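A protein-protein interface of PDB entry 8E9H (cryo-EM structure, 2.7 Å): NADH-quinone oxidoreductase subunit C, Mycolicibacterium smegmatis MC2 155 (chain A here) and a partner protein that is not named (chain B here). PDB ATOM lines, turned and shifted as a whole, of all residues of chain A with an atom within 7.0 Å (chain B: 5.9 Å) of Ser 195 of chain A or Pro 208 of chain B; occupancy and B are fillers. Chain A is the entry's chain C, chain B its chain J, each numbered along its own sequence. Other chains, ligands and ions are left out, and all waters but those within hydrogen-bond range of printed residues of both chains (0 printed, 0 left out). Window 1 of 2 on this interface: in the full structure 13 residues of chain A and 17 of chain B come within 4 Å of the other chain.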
ATOM      1  N   ASP A 176     -17.468 -15.679   2.502  1.00  0.00           N
ATOM      2  CA  ASP A 176     -17.093 -16.619   3.540  1.00  0.00           C
ATOM      3  C   ASP A 176     -15.839 -16.122   4.249  1.00  0.00           C
ATOM      4  O   ASP A 176     -14.947 -15.528   3.644  1.00  0.00           O
ATOM      5  CB  ASP A 176     -16.856 -18.007   2.954  1.00  0.00           C
ATOM      6  CG  ASP A 176     -16.843 -19.081   4.012  1.00  0.00           C
ATOM      7  OD1 ASP A 176     -17.144 -18.761   5.177  1.00  0.00           O
ATOM      8  OD2 ASP A 176     -16.532 -20.243   3.681  1.00  0.00           O
ATOM      9  N   TRP A 177     -15.799 -16.352   5.557  1.00  0.00           N
ATOM     10  CA  TRP A 177     -14.796 -15.790   6.457  1.00  0.00           C
ATOM     11  C   TRP A 177     -15.047 -14.312   6.709  1.00  0.00           C
ATOM     12  O   TRP A 177     -14.461 -13.734   7.626  1.00  0.00           O
ATOM     13  CB  TRP A 177     -13.374 -15.945   5.920  1.00  0.00           C
ATOM     14  CG  TRP A 177     -12.871 -17.330   5.860  1.00  0.00           C
ATOM     15  CD1 TRP A 177     -13.601 -18.471   5.768  1.00  0.00           C
ATOM     16  CD2 TRP A 177     -11.503 -17.727   5.905  1.00  0.00           C
ATOM     17  NE1 TRP A 177     -12.770 -19.562   5.744  1.00  0.00           N
ATOM     18  CE2 TRP A 177     -11.474 -19.127   5.829  1.00  0.00           C
ATOM     19  CE3 TRP A 177     -10.299 -17.031   6.001  1.00  0.00           C
ATOM     20  CZ2 TRP A 177     -10.287 -19.844   5.844  1.00  0.00           C
ATOM     21  CZ3 TRP A 177      -9.126 -17.742   6.017  1.00  0.00           C
ATOM     22  CH2 TRP A 177      -9.125 -19.133   5.938  1.00  0.00           C
ATOM     23  N   ARG A 180     -18.606 -15.144   8.397  1.00  0.00           N
ATOM     24  CA  ARG A 180     -18.244 -15.803   9.648  1.00  0.00           C
ATOM     25  C   ARG A 180     -17.681 -14.809  10.654  1.00  0.00           C
ATOM     26  O   ARG A 180     -18.056 -14.830  11.830  1.00  0.00           O
ATOM     27  CB  ARG A 180     -17.239 -16.920   9.378  1.00  0.00           C
ATOM     28  CG  ARG A 180     -17.869 -18.175   8.813  1.00  0.00           C
ATOM     29  CD  ARG A 180     -16.843 -19.252   8.542  1.00  0.00           C
ATOM     30  NE  ARG A 180     -16.151 -19.671   9.753  1.00  0.00           N
ATOM     31  CZ  ARG A 180     -14.960 -20.250   9.773  1.00  0.00           C
ATOM     32  NH1 ARG A 180     -14.307 -20.530   8.658  1.00  0.00           N
ATOM     33  NH2 ARG A 180     -14.410 -20.560  10.942  1.00  0.00           N
ATOM     34  N   GLY A 192     -28.109 -19.496   5.082  1.00  0.00           N
ATOM     35  CA  GLY A 192     -27.645 -20.017   3.818  1.00  0.00           C
ATOM     36  C   GLY A 192     -26.146 -20.151   3.713  1.00  0.00           C
ATOM     37  O   GLY A 192     -25.658 -20.714   2.728  1.00  0.00           O
ATOM     38  N   HIS A 193     -25.402 -19.654   4.690  1.00  0.00           N
ATOM     39  CA  HIS A 193     -23.959 -19.791   4.669  1.00  0.00           C
ATOM     40  C   HIS A 193     -23.583 -21.254   4.901  1.00  0.00           C
ATOM     41  O   HIS A 193     -24.192 -21.923   5.740  1.00  0.00           O
ATOM     42  CB  HIS A 193     -23.339 -18.901   5.743  1.00  0.00           C
ATOM     43  CG  HIS A 193     -21.845 -18.907   5.749  1.00  0.00           C
ATOM     44  ND1 HIS A 193     -21.109 -19.924   6.310  1.00  0.00           N
ATOM     45  CD2 HIS A 193     -20.950 -18.014   5.266  1.00  0.00           C
ATOM     46  CE1 HIS A 193     -19.822 -19.660   6.172  1.00  0.00           C
ATOM     47  NE2 HIS A 193     -19.699 -18.508   5.541  1.00  0.00           N
ATOM     48  N   PRO A 194     -22.595 -21.783   4.173  1.00  0.00           N
ATOM     49  CA  PRO A 194     -22.297 -23.218   4.302  1.00  0.00           C
ATOM     50  C   PRO A 194     -22.059 -23.659   5.731  1.00  0.00           C
ATOM     51  O   PRO A 194     -22.571 -24.707   6.141  1.00  0.00           O
ATOM     52  CB  PRO A 194     -21.035 -23.389   3.448  1.00  0.00           C
ATOM     53  CG  PRO A 194     -21.079 -22.280   2.481  1.00  0.00           C
ATOM     54  CD  PRO A 194     -21.716 -21.129   3.190  1.00  0.00           C
ATOM     55  N   SER A 195     -21.296 -22.892   6.504  1.00  0.00           N
ATOM     56  CA  SER A 195     -21.118 -23.169   7.921  1.00  0.00           C
ATOM     57  C   SER A 195     -20.756 -21.888   8.654  1.00  0.00           C
ATOM     58  O   SER A 195     -19.604 -21.448   8.613  1.00  0.00           O
ATOM     59  CB  SER A 195     -20.039 -24.227   8.130  1.00  0.00           C
ATOM     60  OG  SER A 195     -20.449 -25.471   7.594  1.00  0.00           O
ATOM     61  N   LEU A 196     -21.732 -21.281   9.326  1.00  0.00           N
ATOM     62  CA  LEU A 196     -21.525 -19.996   9.990  1.00  0.00           C
ATOM     63  C   LEU A 196     -20.975 -20.209  11.400  1.00  0.00           C
ATOM     64  O   LEU A 196     -21.630 -19.956  12.409  1.00  0.00           O
ATOM     65  CB  LEU A 196     -22.822 -19.204  10.014  1.00  0.00           C
ATOM     66  CG  LEU A 196     -22.639 -17.707  10.249  1.00  0.00           C
ATOM     67  CD1 LEU A 196     -22.048 -17.046   9.020  1.00  0.00           C
ATOM     68  CD2 LEU A 196     -23.957 -17.068  10.620  1.00  0.00           C
ATOM     69  N   THR A 197     -19.740 -20.688  11.450  1.00  0.00           N
ATOM     70  CA  THR A 197     -19.072 -20.923  12.716  1.00  0.00           C
ATOM     71  C   THR A 197     -18.143 -19.763  13.050  1.00  0.00           C
ATOM     72  O   THR A 197     -17.673 -19.036  12.172  1.00  0.00           O
ATOM     73  CB  THR A 197     -18.278 -22.224  12.665  1.00  0.00           C
ATOM     74  OG1 THR A 197     -17.234 -22.107  11.692  1.00  0.00           O
ATOM     75  CG2 THR A 197     -19.181 -23.377  12.285  1.00  0.00           C
ATOM     76  N   ARG A 198     -17.874 -19.598  14.340  1.00  0.00           N
ATOM     77  CA  ARG A 198     -16.939 -18.574  14.770  1.00  0.00           C
ATOM     78  C   ARG A 198     -15.569 -18.822  14.154  1.00  0.00           C
ATOM     79  O   ARG A 198     -15.122 -19.961  14.003  1.00  0.00           O
ATOM     80  CB  ARG A 198     -16.829 -18.552  16.291  1.00  0.00           C
ATOM     81  CG  ARG A 198     -18.049 -18.000  16.985  1.00  0.00           C
ATOM     82  CD  ARG A 198     -17.802 -17.829  18.464  1.00  0.00           C
ATOM     83  NE  ARG A 198     -19.002 -17.398  19.168  1.00  0.00           N
ATOM     84  CZ  ARG A 198     -19.278 -16.142  19.494  1.00  0.00           C
ATOM     85  NH1 ARG A 198     -18.456 -15.151  19.194  1.00  0.00           N
ATOM     86  NH2 ARG A 198     -20.409 -15.874  20.136  1.00  0.00           N
ATOM     87  N   PRO B 204     -17.290 -24.585  -0.207  1.00  0.00           N
ATOM     88  CA  PRO B 204     -16.885 -24.042   1.099  1.00  0.00           C
ATOM     89  C   PRO B 204     -15.479 -23.463   1.227  1.00  0.00           C
ATOM     90  O   PRO B 204     -14.815 -23.742   2.230  1.00  0.00           O
ATOM     91  CB  PRO B 204     -17.053 -25.260   2.011  1.00  0.00           C
ATOM     92  CG  PRO B 204     -18.218 -26.024   1.392  1.00  0.00           C
ATOM     93  CD  PRO B 204     -18.376 -25.562  -0.048  1.00  0.00           C
ATOM     94  N   PRO B 206     -11.912 -22.518   1.918  1.00  0.00           N
ATOM     95  CA  PRO B 206     -11.378 -23.516   2.854  1.00  0.00           C
ATOM     96  C   PRO B 206     -12.483 -23.971   3.795  1.00  0.00           C
ATOM     97  O   PRO B 206     -13.162 -23.148   4.411  1.00  0.00           O
ATOM     98  CB  PRO B 206     -10.275 -22.757   3.595  1.00  0.00           C
ATOM     99  CG  PRO B 206      -9.869 -21.704   2.672  1.00  0.00           C
ATOM    100  CD  PRO B 206     -11.110 -21.285   1.963  1.00  0.00           C
ATOM    101  N   LEU B 207     -12.677 -25.278   3.887  1.00  0.00           N
ATOM    102  CA  LEU B 207     -13.716 -25.825   4.746  1.00  0.00           C
ATOM    103  C   LEU B 207     -13.566 -25.243   6.145  1.00  0.00           C
ATOM    104  O   LEU B 207     -12.453 -24.897   6.554  1.00  0.00           O
ATOM    105  CB  LEU B 207     -13.635 -27.348   4.779  1.00  0.00           C
ATOM    106  CG  LEU B 207     -14.064 -28.048   3.491  1.00  0.00           C
ATOM    107  CD1 LEU B 207     -13.575 -29.478   3.487  1.00  0.00           C
ATOM    108  CD2 LEU B 207     -15.570 -28.014   3.335  1.00  0.00           C
ATOM    109  N   PRO B 208     -14.652 -25.110   6.901  1.00  0.00           N
ATOM    110  CA  PRO B 208     -14.548 -24.485   8.221  1.00  0.00           C
ATOM    111  C   PRO B 208     -13.562 -25.222   9.110  1.00  0.00           C
ATOM    112  O   PRO B 208     -13.455 -26.449   9.078  1.00  0.00           O
ATOM    113  CB  PRO B 208     -15.975 -24.574   8.771  1.00  0.00           C
ATOM    114  CG  PRO B 208     -16.630 -25.638   7.972  1.00  0.00           C
ATOM    115  CD  PRO B 208     -16.019 -25.566   6.618  1.00  0.00           C
ATOM    116  N   ASN B 209     -12.837 -24.452   9.912  1.00  0.00           N
ATOM    117  CA  ASN B 209     -11.854 -25.007  10.817  1.00  0.00           C
ATOM    118  C   ASN B 209     -12.545 -25.850  11.879  1.00  0.00           C
ATOM    119  O   ASN B 209     -13.720 -25.644  12.183  1.00  0.00           O
ATOM    120  CB  ASN B 209     -11.059 -23.885  11.477  1.00  0.00           C
ATOM    121  CG  ASN B 209     -11.942 -22.936  12.262  1.00  0.00           C
ATOM    122  OD1 ASN B 209     -13.158 -23.109  12.313  1.00  0.00           O
ATOM    123  ND2 ASN B 209     -11.339 -21.931  12.877  1.00  0.00           N
ATOM    124  N   PRO B 210     -11.845 -26.816  12.461  1.00  0.00           N
ATOM    125  CA  PRO B 210     -12.398 -27.516  13.619  1.00  0.00           C
ATOM    126  C   PRO B 210     -12.583 -26.561  14.784  1.00  0.00           C
ATOM    127  O   PRO B 210     -11.825 -25.609  14.973  1.00  0.00           O
ATOM    128  CB  PRO B 210     -11.348 -28.584  13.930  1.00  0.00           C
ATOM    129  CG  PRO B 210     -10.098 -28.068  13.338  1.00  0.00           C
ATOM    130  CD  PRO B 210     -10.501 -27.306  12.119  1.00  0.00           C
ATOM    131  N   ALA B 223     -16.841 -27.720  15.062  1.00  0.00           N
ATOM    132  CA  ALA B 223     -17.186 -26.327  15.290  1.00  0.00           C
ATOM    133  C   ALA B 223     -18.675 -26.190  15.584  1.00  0.00           C
ATOM    134  O   ALA B 223     -19.490 -27.040  15.220  1.00  0.00           O
ATOM    135  CB  ALA B 223     -16.812 -25.474  14.081  1.00  0.00           C
ATOM    136  N   LEU B 225     -22.250 -24.363  15.256  1.00  0.00           N
ATOM    137  CA  LEU B 225     -23.081 -23.514  14.424  1.00  0.00           C
ATOM    138  C   LEU B 225     -23.855 -22.528  15.292  1.00  0.00           C
ATOM    139  O   LEU B 225     -23.961 -22.705  16.506  1.00  0.00           O
ATOM    140  CB  LEU B 225     -24.044 -24.360  13.599  1.00  0.00           C
ATOM    141  CG  LEU B 225     -23.404 -25.218  12.510  1.00  0.00           C
ATOM    142  CD1 LEU B 225     -24.429 -26.158  11.910  1.00  0.00           C
ATOM    143  CD2 LEU B 225     -22.787 -24.348  11.432  1.00  0.00           C
ATOM    144  N   SER B 231     -21.055 -28.339  13.543  1.00  0.00           N
ATOM    145  CA  SER B 231     -20.995 -28.182  12.096  1.00  0.00           C
ATOM    146  C   SER B 231     -20.393 -29.431  11.465  1.00  0.00           C
ATOM    147  O   SER B 231     -19.240 -29.765  11.762  1.00  0.00           O
ATOM    148  CB  SER B 231     -20.165 -26.960  11.731  1.00  0.00           C
ATOM    149  OG  SER B 231     -19.845 -26.962  10.353  1.00  0.00           O
ATOM    150  N   PRO B 232     -21.119 -30.147  10.602  1.00  0.00           N
ATOM    151  CA  PRO B 232     -20.526 -31.353  10.003  1.00  0.00           C
ATOM    152  C   PRO B 232     -19.269 -31.073   9.203  1.00  0.00           C
ATOM    153  O   PRO B 232     -18.323 -31.867   9.246  1.00  0.00           O
ATOM    154  CB  PRO B 232     -21.655 -31.893   9.114  1.00  0.00           C
ATOM    155  CG  PRO B 232     -22.897 -31.266   9.640  1.00  0.00           C
ATOM    156  CD  PRO B 232     -22.490 -29.919  10.122  1.00  0.00           C
ATOM    157  N   LEU B 233     -19.228 -29.960   8.471  1.00  0.00           N
ATOM    158  CA  LEU B 233     -18.078 -29.670   7.626  1.00  0.00           C
ATOM    159  C   LEU B 233     -16.835 -29.335   8.434  1.00  0.00           C
ATOM    160  O   LEU B 233     -15.723 -29.442   7.908  1.00  0.00           O
ATOM    161  CB  LEU B 233     -18.397 -28.508   6.688  1.00  0.00           C
ATOM    162  CG  LEU B 233     -19.525 -28.734   5.682  1.00  0.00           C
ATOM    163  CD1 LEU B 233     -19.721 -27.495   4.832  1.00  0.00           C
ATOM    164  CD2 LEU B 233     -19.240 -29.938   4.806  1.00  0.00           C
ATOM    165  N   SER B 234     -16.994 -28.932   9.692  1.00  0.00           N
ATOM    166  CA  SER B 234     -15.858 -28.451  10.465  1.00  0.00           C
ATOM    167  C   SER B 234     -14.813 -29.528  10.703  1.00  0.00           C
ATOM    168  O   SER B 234     -13.631 -29.202  10.839  1.00  0.00           O
ATOM    169  CB  SER B 234     -16.340 -27.900  11.802  1.00  0.00           C
ATOM    170  OG  SER B 234     -16.825 -28.939  12.628  1.00  0.00           O
ATOM    171  N   VAL B 235     -15.210 -30.796  10.748  1.00  0.00           N
ATOM    172  CA  VAL B 235     -14.300 -31.894  11.045  1.00  0.00           C
ATOM    173  C   VAL B 235     -14.281 -32.837   9.855  1.00  0.00           C
ATOM    174  O   VAL B 235     -15.336 -33.171   9.304  1.00  0.00           O
ATOM    175  CB  VAL B 235     -14.709 -32.644  12.326  1.00  0.00           C
ATOM    176  CG1 VAL B 235     -16.057 -33.315  12.143  1.00  0.00           C
ATOM    177  CG2 VAL B 235     -13.651 -33.662  12.698  1.00  0.00           C
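NH2 of Arg 180 of chain A lies within hydrogen-bond range of OD1 of Asn 209 of chain B (3.2 Å). OG of Ser 231 of chain B is in hydrogen-bond range of OG of Ser 195 of chain A, 3.2 Å away.
The side-chain hydroxyl (OG) of Ser 234 of chain B sits at hydrogen-bond distance from the backbone NH (N) of Ala 223 of chain B, 2.7 Å away. O of Ser 231 of chain B lies within hydrogen-bond range of OG of Ser 234 of chain B (2.7 Å). The guanidinium group (NE) of Arg 180 of chain A sits at hydrogen-bond distance from the backbone carbonyl oxygen (O) of Thr 197 of chain A (2.9 Å). The guanidinium group (NH2) of Arg 180 of chain A lies within hydrogen-bond range of the backbone carbonyl oxygen (O) of Arg 198 of chain A. ND1 of His 193 of chain A lies within hydrogen-bond range of N of Ser 195 of chain A, 3.0 Å away. A ring nitrogen (ND1) of His 193 of chain A is in hydrogen-bond range of the backbone NH (N) of Leu 196 of chain A (3.4 Å).
Among the printed residues, pairs that only touch across the chains: Trp 177 of chain A with Pro 206 of chain B (3.7 Å), Arg 180 of chain A with Pro 208 of chain B (3.99 Å), Ser 195 of chain A with Pro 208 of chain B (3.7 Å), Ser 195 of chain A with Leu 233 of chain B (3.5 Å), Leu 196 of chain A with Leu 225 of chain B (3.9 Å), Thr 197 of chain A with Ala 223 of chain B (3.6 Å), Thr 197 of chain A with Leu 225 of chain B (3.8 Å) and Thr 197 of chain A with Ser 231 of chain B (3.8 Å).
Ser 195 of chain A touches just these residues of chain B: Pro 208, Ser 231 and Leu 233. Printed residues of chain A within 4 Å of Pro 208 of chain B: Arg 180 (3.99 Å) and Ser 195 (3.7 Å). Of the printed residues of chain B, Trp 177 of chain A touches Pro 206. Of the printed residues of chain A, Ser 231 of chain B touches Ser 195 (3.2 Å) and Thr 197 (3.8 Å). Printed residues of chain A within 4 Å of Leu 233 of chain B: Ser 195 (3.5 Å). Printed residues of chain A within 4 Å of Pro 206 of chain B: Trp 177 (3.7 Å). Of the printed residues of chain A, Ala 223 of chain B touches Thr 197 (3.6 Å). The nearest residue of chain B that does not touch Ser 195 of chain A is Leu 225 of chain B (4.1 Å).
Hydrophobic or aromatic side chains of chain A within 4 Å of the printed part of chain B: Trp 177. Printed residues of chain B that touch a printed residue of chain A: Pro 206, Pro 208, Asn 209, Ala 223, Leu 225, Ser 231 and Leu 233. Hydrophobic or aromatic side chains of chain B that line the printed part of chain A: Pro 206, Pro 208, Ala 223, Leu 225 and Leu 233. Among the printed residues, 10 pairs touch across the chains.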
